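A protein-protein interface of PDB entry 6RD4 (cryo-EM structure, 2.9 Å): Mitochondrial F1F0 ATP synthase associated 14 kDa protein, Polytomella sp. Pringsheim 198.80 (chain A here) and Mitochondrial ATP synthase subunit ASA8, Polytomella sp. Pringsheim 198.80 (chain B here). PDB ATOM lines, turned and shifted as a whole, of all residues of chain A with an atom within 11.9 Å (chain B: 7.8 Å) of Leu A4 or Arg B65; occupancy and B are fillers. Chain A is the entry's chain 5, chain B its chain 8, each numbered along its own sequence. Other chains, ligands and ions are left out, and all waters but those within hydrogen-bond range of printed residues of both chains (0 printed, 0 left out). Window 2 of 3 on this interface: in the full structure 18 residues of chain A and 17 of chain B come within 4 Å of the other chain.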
ATOM      1  N   MET A   1      -4.631  -3.545 -17.070  1.00  0.00           N
ATOM      2  CA  MET A   1      -4.985  -4.780 -17.750  1.00  0.00           C
ATOM      3  C   MET A   1      -5.141  -5.916 -16.754  1.00  0.00           C
ATOM      4  O   MET A   1      -5.227  -5.694 -15.548  1.00  0.00           O
ATOM      5  CB  MET A   1      -3.930  -5.126 -18.804  1.00  0.00           C
ATOM      6  CG  MET A   1      -2.523  -5.271 -18.247  1.00  0.00           C
ATOM      7  SD  MET A   1      -1.209  -4.890 -19.416  1.00  0.00           S
ATOM      8  CE  MET A   1      -1.785  -3.326 -20.076  1.00  0.00           C
ATOM      9  N   LYS A   2      -5.190  -7.136 -17.274  1.00  0.00           N
ATOM     10  CA  LYS A   2      -5.292  -8.334 -16.448  1.00  0.00           C
ATOM     11  C   LYS A   2      -3.928  -8.624 -15.842  1.00  0.00           C
ATOM     12  O   LYS A   2      -3.004  -9.026 -16.551  1.00  0.00           O
ATOM     13  CB  LYS A   2      -5.782  -9.510 -17.289  1.00  0.00           C
ATOM     14  CG  LYS A   2      -5.838 -10.830 -16.563  1.00  0.00           C
ATOM     15  CD  LYS A   2      -6.986 -10.868 -15.583  1.00  0.00           C
ATOM     16  CE  LYS A   2      -7.202 -12.267 -15.040  1.00  0.00           C
ATOM     17  NZ  LYS A   2      -7.534 -13.245 -16.106  1.00  0.00           N
ATOM     18  N   LEU A   3      -3.786  -8.391 -14.542  1.00  0.00           N
ATOM     19  CA  LEU A   3      -2.584  -8.777 -13.823  1.00  0.00           C
ATOM     20  C   LEU A   3      -2.850  -9.886 -12.821  1.00  0.00           C
ATOM     21  O   LEU A   3      -2.319 -10.983 -12.974  1.00  0.00           O
ATOM     22  CB  LEU A   3      -1.964  -7.579 -13.109  1.00  0.00           C
ATOM     23  CG  LEU A   3      -0.762  -6.918 -13.757  1.00  0.00           C
ATOM     24  CD1 LEU A   3      -1.143  -6.146 -14.973  1.00  0.00           C
ATOM     25  CD2 LEU A   3      -0.140  -6.024 -12.723  1.00  0.00           C
ATOM     26  N   LEU A   4      -3.676  -9.635 -11.832  1.00  0.00           N
ATOM     27  CA  LEU A   4      -3.872 -10.783 -10.968  1.00  0.00           C
ATOM     28  C   LEU A   4      -5.052 -11.599 -11.463  1.00  0.00           C
ATOM     29  O   LEU A   4      -6.011 -11.041 -11.988  1.00  0.00           O
ATOM     30  CB  LEU A   4      -4.111 -10.355  -9.532  1.00  0.00           C
ATOM     31  CG  LEU A   4      -2.842 -10.264  -8.703  1.00  0.00           C
ATOM     32  CD1 LEU A   4      -2.146  -8.960  -8.920  1.00  0.00           C
ATOM     33  CD2 LEU A   4      -3.135 -10.454  -7.264  1.00  0.00           C
ATOM     34  N   PRO A   5      -4.998 -12.910 -11.361  1.00  0.00           N
ATOM     35  CA  PRO A   5      -6.126 -13.731 -11.775  1.00  0.00           C
ATOM     36  C   PRO A   5      -7.227 -13.699 -10.728  1.00  0.00           C
ATOM     37  O   PRO A   5      -7.111 -13.082  -9.678  1.00  0.00           O
ATOM     38  CB  PRO A   5      -5.503 -15.111 -11.907  1.00  0.00           C
ATOM     39  CG  PRO A   5      -4.385 -15.093 -10.994  1.00  0.00           C
ATOM     40  CD  PRO A   5      -3.837 -13.733 -11.007  1.00  0.00           C
ATOM     41  N   GLU A   6      -8.326 -14.364 -11.056  1.00  0.00           N
ATOM     42  CA  GLU A   6      -9.427 -14.479 -10.119  1.00  0.00           C
ATOM     43  C   GLU A   6      -9.062 -15.381  -8.951  1.00  0.00           C
ATOM     44  O   GLU A   6      -9.471 -15.124  -7.815  1.00  0.00           O
ATOM     45  CB  GLU A   6     -10.656 -14.986 -10.864  1.00  0.00           C
ATOM     46  CG  GLU A   6     -11.884 -15.178 -10.031  1.00  0.00           C
ATOM     47  CD  GLU A   6     -12.810 -16.199 -10.642  1.00  0.00           C
ATOM     48  OE1 GLU A   6     -13.715 -16.682  -9.935  1.00  0.00           O
ATOM     49  OE2 GLU A   6     -12.632 -16.519 -11.835  1.00  0.00           O
ATOM     50  N   SER A   7      -8.274 -16.414  -9.202  1.00  0.00           N
ATOM     51  CA  SER A   7      -7.693 -17.219  -8.138  1.00  0.00           C
ATOM     52  C   SER A   7      -6.259 -17.512  -8.518  1.00  0.00           C
ATOM     53  O   SER A   7      -6.003 -17.977  -9.625  1.00  0.00           O
ATOM     54  CB  SER A   7      -8.463 -18.510  -7.932  1.00  0.00           C
ATOM     55  OG  SER A   7      -8.111 -19.118  -6.711  1.00  0.00           O
ATOM     56  N   LEU A   8      -5.326 -17.218  -7.622  1.00  0.00           N
ATOM     57  CA  LEU A   8      -3.941 -17.568  -7.877  1.00  0.00           C
ATOM     58  C   LEU A   8      -3.694 -19.041  -7.648  1.00  0.00           C
ATOM     59  O   LEU A   8      -2.807 -19.617  -8.269  1.00  0.00           O
ATOM     60  CB  LEU A   8      -3.013 -16.763  -6.985  1.00  0.00           C
ATOM     61  CG  LEU A   8      -2.622 -15.358  -7.391  1.00  0.00           C
ATOM     62  CD1 LEU A   8      -2.113 -14.678  -6.169  1.00  0.00           C
ATOM     63  CD2 LEU A   8      -1.572 -15.384  -8.441  1.00  0.00           C
ATOM     64  N   GLN A   9      -4.438 -19.657  -6.736  1.00  0.00           N
ATOM     65  CA  GLN A   9      -4.275 -21.077  -6.484  1.00  0.00           C
ATOM     66  C   GLN A   9      -4.839 -21.904  -7.618  1.00  0.00           C
ATOM     67  O   GLN A   9      -4.372 -23.011  -7.861  1.00  0.00           O
ATOM     68  CB  GLN A   9      -4.964 -21.453  -5.189  1.00  0.00           C
ATOM     69  CG  GLN A   9      -4.594 -22.774  -4.644  1.00  0.00           C
ATOM     70  CD  GLN A   9      -5.278 -23.038  -3.356  1.00  0.00           C
ATOM     71  OE1 GLN A   9      -6.467 -22.822  -3.235  1.00  0.00           O
ATOM     72  NE2 GLN A   9      -4.533 -23.489  -2.373  1.00  0.00           N
ATOM     73  N   GLN A  10      -5.844 -21.400  -8.313  1.00  0.00           N
ATOM     74  CA  GLN A  10      -6.382 -22.134  -9.440  1.00  0.00           C
ATOM     75  C   GLN A  10      -5.435 -22.091 -10.622  1.00  0.00           C
ATOM     76  O   GLN A  10      -5.355 -23.050 -11.389  1.00  0.00           O
ATOM     77  CB  GLN A  10      -7.733 -21.560  -9.816  1.00  0.00           C
ATOM     78  CG  GLN A  10      -8.438 -22.264 -10.908  1.00  0.00           C
ATOM     79  CD  GLN A  10      -9.351 -21.362 -11.638  1.00  0.00           C
ATOM     80  OE1 GLN A  10      -9.188 -20.155 -11.618  1.00  0.00           O
ATOM     81  NE2 GLN A  10     -10.329 -21.931 -12.291  1.00  0.00           N
ATOM     82  N   GLU A  11      -4.717 -20.988 -10.801  1.00  0.00           N
ATOM     83  CA  GLU A  11      -3.718 -20.946 -11.853  1.00  0.00           C
ATOM     84  C   GLU A  11      -2.435 -21.646 -11.477  1.00  0.00           C
ATOM     85  O   GLU A  11      -1.739 -22.143 -12.356  1.00  0.00           O
ATOM     86  CB  GLU A  11      -3.395 -19.519 -12.241  1.00  0.00           C
ATOM     87  CG  GLU A  11      -4.346 -18.896 -13.192  1.00  0.00           C
ATOM     88  CD  GLU A  11      -3.796 -17.601 -13.742  1.00  0.00           C
ATOM     89  OE1 GLU A  11      -2.790 -17.121 -13.200  1.00  0.00           O
ATOM     90  OE2 GLU A  11      -4.331 -17.078 -14.735  1.00  0.00           O
ATOM     91  N   ALA A  12      -2.071 -21.663 -10.208  1.00  0.00           N
ATOM     92  CA  ALA A  12      -0.903 -22.423  -9.811  1.00  0.00           C
ATOM     93  C   ALA A  12      -1.166 -23.907  -9.877  1.00  0.00           C
ATOM     94  O   ALA A  12      -0.254 -24.672 -10.176  1.00  0.00           O
ATOM     95  CB  ALA A  12      -0.474 -22.048  -8.403  1.00  0.00           C
ATOM     96  N   TYR B  58       0.158 -20.254  -2.641  1.00  0.00           N
ATOM     97  CA  TYR B  58      -0.732 -19.392  -3.390  1.00  0.00           C
ATOM     98  C   TYR B  58      -2.139 -19.445  -2.846  1.00  0.00           C
ATOM     99  O   TYR B  58      -2.963 -18.617  -3.221  1.00  0.00           O
ATOM    100  CB  TYR B  58      -0.738 -19.774  -4.857  1.00  0.00           C
ATOM    101  CG  TYR B  58       0.374 -19.185  -5.669  1.00  0.00           C
ATOM    102  CD1 TYR B  58       1.658 -19.125  -5.190  1.00  0.00           C
ATOM    103  CD2 TYR B  58       0.136 -18.703  -6.921  1.00  0.00           C
ATOM    104  CE1 TYR B  58       2.660 -18.600  -5.934  1.00  0.00           C
ATOM    105  CE2 TYR B  58       1.131 -18.180  -7.668  1.00  0.00           C
ATOM    106  CZ  TYR B  58       2.383 -18.133  -7.169  1.00  0.00           C
ATOM    107  OH  TYR B  58       3.373 -17.602  -7.924  1.00  0.00           O
ATOM    108  N   GLY B  59      -2.437 -20.413  -1.989  1.00  0.00           N
ATOM    109  CA  GLY B  59      -3.653 -20.382  -1.211  1.00  0.00           C
ATOM    110  C   GLY B  59      -3.553 -19.556   0.043  1.00  0.00           C
ATOM    111  O   GLY B  59      -4.580 -19.146   0.581  1.00  0.00           O
ATOM    112  N   ILE B  60      -2.339 -19.327   0.539  1.00  0.00           N
ATOM    113  CA  ILE B  60      -2.135 -18.299   1.548  1.00  0.00           C
ATOM    114  C   ILE B  60      -2.371 -16.930   0.939  1.00  0.00           C
ATOM    115  O   ILE B  60      -3.092 -16.106   1.497  1.00  0.00           O
ATOM    116  CB  ILE B  60      -0.723 -18.395   2.148  1.00  0.00           C
ATOM    117  CG1 ILE B  60      -0.425 -19.784   2.695  1.00  0.00           C
ATOM    118  CG2 ILE B  60      -0.546 -17.392   3.226  1.00  0.00           C
ATOM    119  CD1 ILE B  60      -1.405 -20.294   3.641  1.00  0.00           C
ATOM    120  N   LEU B  61      -1.788 -16.678  -0.231  1.00  0.00           N
ATOM    121  CA  LEU B  61      -1.904 -15.375  -0.868  1.00  0.00           C
ATOM    122  C   LEU B  61      -3.296 -15.125  -1.417  1.00  0.00           C
ATOM    123  O   LEU B  61      -3.677 -13.976  -1.619  1.00  0.00           O
ATOM    124  CB  LEU B  61      -0.894 -15.246  -1.997  1.00  0.00           C
ATOM    125  CG  LEU B  61       0.555 -15.530  -1.650  1.00  0.00           C
ATOM    126  CD1 LEU B  61       1.426 -15.327  -2.849  1.00  0.00           C
ATOM    127  CD2 LEU B  61       0.995 -14.655  -0.522  1.00  0.00           C
ATOM    128  N   ASP B  62      -4.051 -16.171  -1.705  1.00  0.00           N
ATOM    129  CA  ASP B  62      -5.448 -15.987  -2.050  1.00  0.00           C
ATOM    130  C   ASP B  62      -6.284 -15.756  -0.812  1.00  0.00           C
ATOM    131  O   ASP B  62      -7.351 -15.144  -0.889  1.00  0.00           O
ATOM    132  CB  ASP B  62      -5.972 -17.207  -2.797  1.00  0.00           C
ATOM    133  CG  ASP B  62      -5.923 -17.044  -4.285  1.00  0.00           C
ATOM    134  OD1 ASP B  62      -5.477 -15.984  -4.755  1.00  0.00           O
ATOM    135  OD2 ASP B  62      -6.356 -17.975  -4.988  1.00  0.00           O
ATOM    136  N   GLY B  63      -5.829 -16.263   0.329  1.00  0.00           N
ATOM    137  CA  GLY B  63      -6.485 -15.973   1.581  1.00  0.00           C
ATOM    138  C   GLY B  63      -6.181 -14.592   2.095  1.00  0.00           C
ATOM    139  O   GLY B  63      -7.032 -13.975   2.736  1.00  0.00           O
ATOM    140  N   LEU B  64      -4.979 -14.085   1.836  1.00  0.00           N
ATOM    141  CA  LEU B  64      -4.661 -12.717   2.221  1.00  0.00           C
ATOM    142  C   LEU B  64      -5.385 -11.717   1.347  1.00  0.00           C
ATOM    143  O   LEU B  64      -5.672 -10.605   1.790  1.00  0.00           O
ATOM    144  CB  LEU B  64      -3.164 -12.455   2.131  1.00  0.00           C
ATOM    145  CG  LEU B  64      -2.198 -13.269   2.973  1.00  0.00           C
ATOM    146  CD1 LEU B  64      -0.862 -12.602   2.962  1.00  0.00           C
ATOM    147  CD2 LEU B  64      -2.690 -13.447   4.367  1.00  0.00           C
ATOM    148  N   ARG B  65      -5.672 -12.085   0.110  1.00  0.00           N
ATOM    149  CA  ARG B  65      -6.317 -11.161  -0.805  1.00  0.00           C
ATOM    150  C   ARG B  65      -7.803 -11.031  -0.518  1.00  0.00           C
ATOM    151  O   ARG B  65      -8.374  -9.959  -0.709  1.00  0.00           O
ATOM    152  CB  ARG B  65      -6.085 -11.614  -2.236  1.00  0.00           C
ATOM    153  CG  ARG B  65      -6.478 -10.609  -3.263  1.00  0.00           C
ATOM    154  CD  ARG B  65      -5.571 -10.681  -4.436  1.00  0.00           C
ATOM    155  NE  ARG B  65      -5.672 -11.967  -5.097  1.00  0.00           N
ATOM    156  CZ  ARG B  65      -6.348 -12.167  -6.220  1.00  0.00           C
ATOM    157  NH1 ARG B  65      -6.386 -13.373  -6.762  1.00  0.00           N
ATOM    158  NH2 ARG B  65      -6.979 -11.160  -6.801  1.00  0.00           N
ATOM    159  N   ASP B  66      -8.456 -12.098  -0.068  1.00  0.00           N
ATOM    160  CA  ASP B  66      -9.856 -11.990   0.321  1.00  0.00           C
ATOM    161  C   ASP B  66     -10.058 -11.494   1.736  1.00  0.00           C
ATOM    162  O   ASP B  66     -11.110 -10.927   2.021  1.00  0.00           O
ATOM    163  CB  ASP B  66     -10.590 -13.319   0.176  1.00  0.00           C
ATOM    164  CG  ASP B  66     -11.320 -13.436  -1.141  1.00  0.00           C
ATOM    165  OD1 ASP B  66     -10.898 -12.823  -2.143  1.00  0.00           O
ATOM    166  OD2 ASP B  66     -12.346 -14.137  -1.168  1.00  0.00           O
ATOM    167  N   SER B  67      -9.101 -11.680   2.631  1.00  0.00           N
ATOM    168  CA  SER B  67      -9.224 -11.020   3.916  1.00  0.00           C
ATOM    169  C   SER B  67      -8.892  -9.543   3.823  1.00  0.00           C
ATOM    170  O   SER B  67      -9.214  -8.793   4.742  1.00  0.00           O
ATOM    171  CB  SER B  67      -8.338 -11.689   4.957  1.00  0.00           C
ATOM    172  OG  SER B  67      -6.978 -11.464   4.675  1.00  0.00           O
ATOM    173  N   GLY B  68      -8.239  -9.114   2.747  1.00  0.00           N
ATOM    174  CA  GLY B  68      -8.093  -7.701   2.479  1.00  0.00           C
ATOM    175  C   GLY B  68      -9.228  -7.107   1.685  1.00  0.00           C
ATOM    176  O   GLY B  68      -9.399  -5.890   1.692  1.00  0.00           O
ATOM    177  N   LYS B  69      -9.976  -7.932   0.964  1.00  0.00           N
ATOM    178  CA  LYS B  69     -11.202  -7.474   0.328  1.00  0.00           C
ATOM    179  C   LYS B  69     -12.314  -7.340   1.344  1.00  0.00           C
ATOM    180  O   LYS B  69     -13.149  -6.445   1.239  1.00  0.00           O
ATOM    181  CB  LYS B  69     -11.634  -8.451  -0.754  1.00  0.00           C
ATOM    182  CG  LYS B  69     -11.141  -8.174  -2.133  1.00  0.00           C
ATOM    183  CD  LYS B  69     -11.652  -9.259  -3.025  1.00  0.00           C
ATOM    184  CE  LYS B  69     -11.366  -8.989  -4.462  1.00  0.00           C
ATOM    185  NZ  LYS B  69     -11.957 -10.067  -5.277  1.00  0.00           N
ATOM    186  N   LYS B  70     -12.358  -8.255   2.305  1.00  0.00           N
ATOM    187  CA  LYS B  70     -13.364  -8.208   3.352  1.00  0.00           C
ATOM    188  C   LYS B  70     -13.117  -7.053   4.295  1.00  0.00           C
ATOM    189  O   LYS B  70     -14.067  -6.471   4.819  1.00  0.00           O
ATOM    190  CB  LYS B  70     -13.350  -9.525   4.112  1.00  0.00           C
ATOM    191  CG  LYS B  70     -14.440  -9.718   5.105  1.00  0.00           C
ATOM    192  CD  LYS B  70     -14.266 -11.048   5.793  1.00  0.00           C
ATOM    193  CE  LYS B  70     -15.306 -11.254   6.871  1.00  0.00           C
ATOM    194  NZ  LYS B  70     -15.246 -10.186   7.894  1.00  0.00           N
ATOM    195  N   LYS B  71     -11.855  -6.701   4.514  1.00  0.00           N
ATOM    196  CA  LYS B  71     -11.538  -5.560   5.362  1.00  0.00           C
ATOM    197  C   LYS B  71     -11.949  -4.255   4.702  1.00  0.00           C
ATOM    198  O   LYS B  71     -12.510  -3.378   5.358  1.00  0.00           O
ATOM    199  CB  LYS B  71     -10.053  -5.580   5.702  1.00  0.00           C
ATOM    200  CG  LYS B  71      -9.412  -4.237   5.934  1.00  0.00           C
ATOM    201  CD  LYS B  71      -8.017  -4.404   6.488  1.00  0.00           C
ATOM    202  CE  LYS B  71      -7.210  -3.135   6.356  1.00  0.00           C
ATOM    203  NZ  LYS B  71      -7.868  -1.981   7.004  1.00  0.00           N
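The backbone carbonyl oxygen (O) of Pro A5 lies within hydrogen-bond range of the guanidinium group (NH1) of Arg B65 (3.0 Å).
The side-chain carboxylate (OD2) of Asp B62 lies within hydrogen-bond range of the side-chain hydroxyl (OG) of Ser A7 (2.7 Å).
N of Leu A8 lies within hydrogen-bond range of OD2 of Asp B62 (2.9 Å).
The side-chain carboxylate (OD2) of Asp B62 sits at hydrogen-bond distance from the backbone NH (N) of Gln A9.
OD1 of Asp B62 lies within salt-bridge range of NH1 of Arg B65, at 3.4 Å.
Leu A4 touches Arg B65.
Glu A6 touches Arg B65.
O of Leu A8 touches CD2 of Tyr B58 (3.4 Å).
Gln A9 touches Tyr B58.
Gly B59 touches Gln A9.
CB of Ala A12 touches CD2 of Tyr B58 (3.7 Å).
Leu A4 touches one residue of chain B.
Of the printed residues of chain B, Glu A6 touches Arg B65 (3.7 Å).
Printed residues of chain B within 4 Å of Gln A9: Tyr B58 (3.95 Å), Gly B59 (3.4 Å) and Asp B62 (3.1 Å).
No residue of chain A comes within 4 Å of Gly B63.
Of chain A, only Leu A4 (3.7 Å), Pro A5 (3.0 Å) and Glu A6 (3.7 Å) come within 4 Å of Arg B65.
No residue of chain A comes within 4 Å of Asp B66.
No residue of chain A comes within 4 Å of Ser B67.
No residue of chain A comes within 4 Å of Gly B68.
No residue of chain A comes within 4 Å of Lys B69.
The nearest printed residue of chain A that does not touch Tyr B58 is Glu A11 (6.0 Å).
Printed residues of chain A that touch a printed residue of chain B: Leu A4, Pro A5, Glu A6, Ser A7, Leu A8, Gln A9 and Ala A12.
Hydrophobic or aromatic side chains of chain A that line the printed part of chain B: Leu A4, Leu A8 and Ala A12.
Along chain A the printed residues that touch a printed residue of chain B span positions 4 to 12.
Among the printed residues, 10 pairs touch across the chains.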
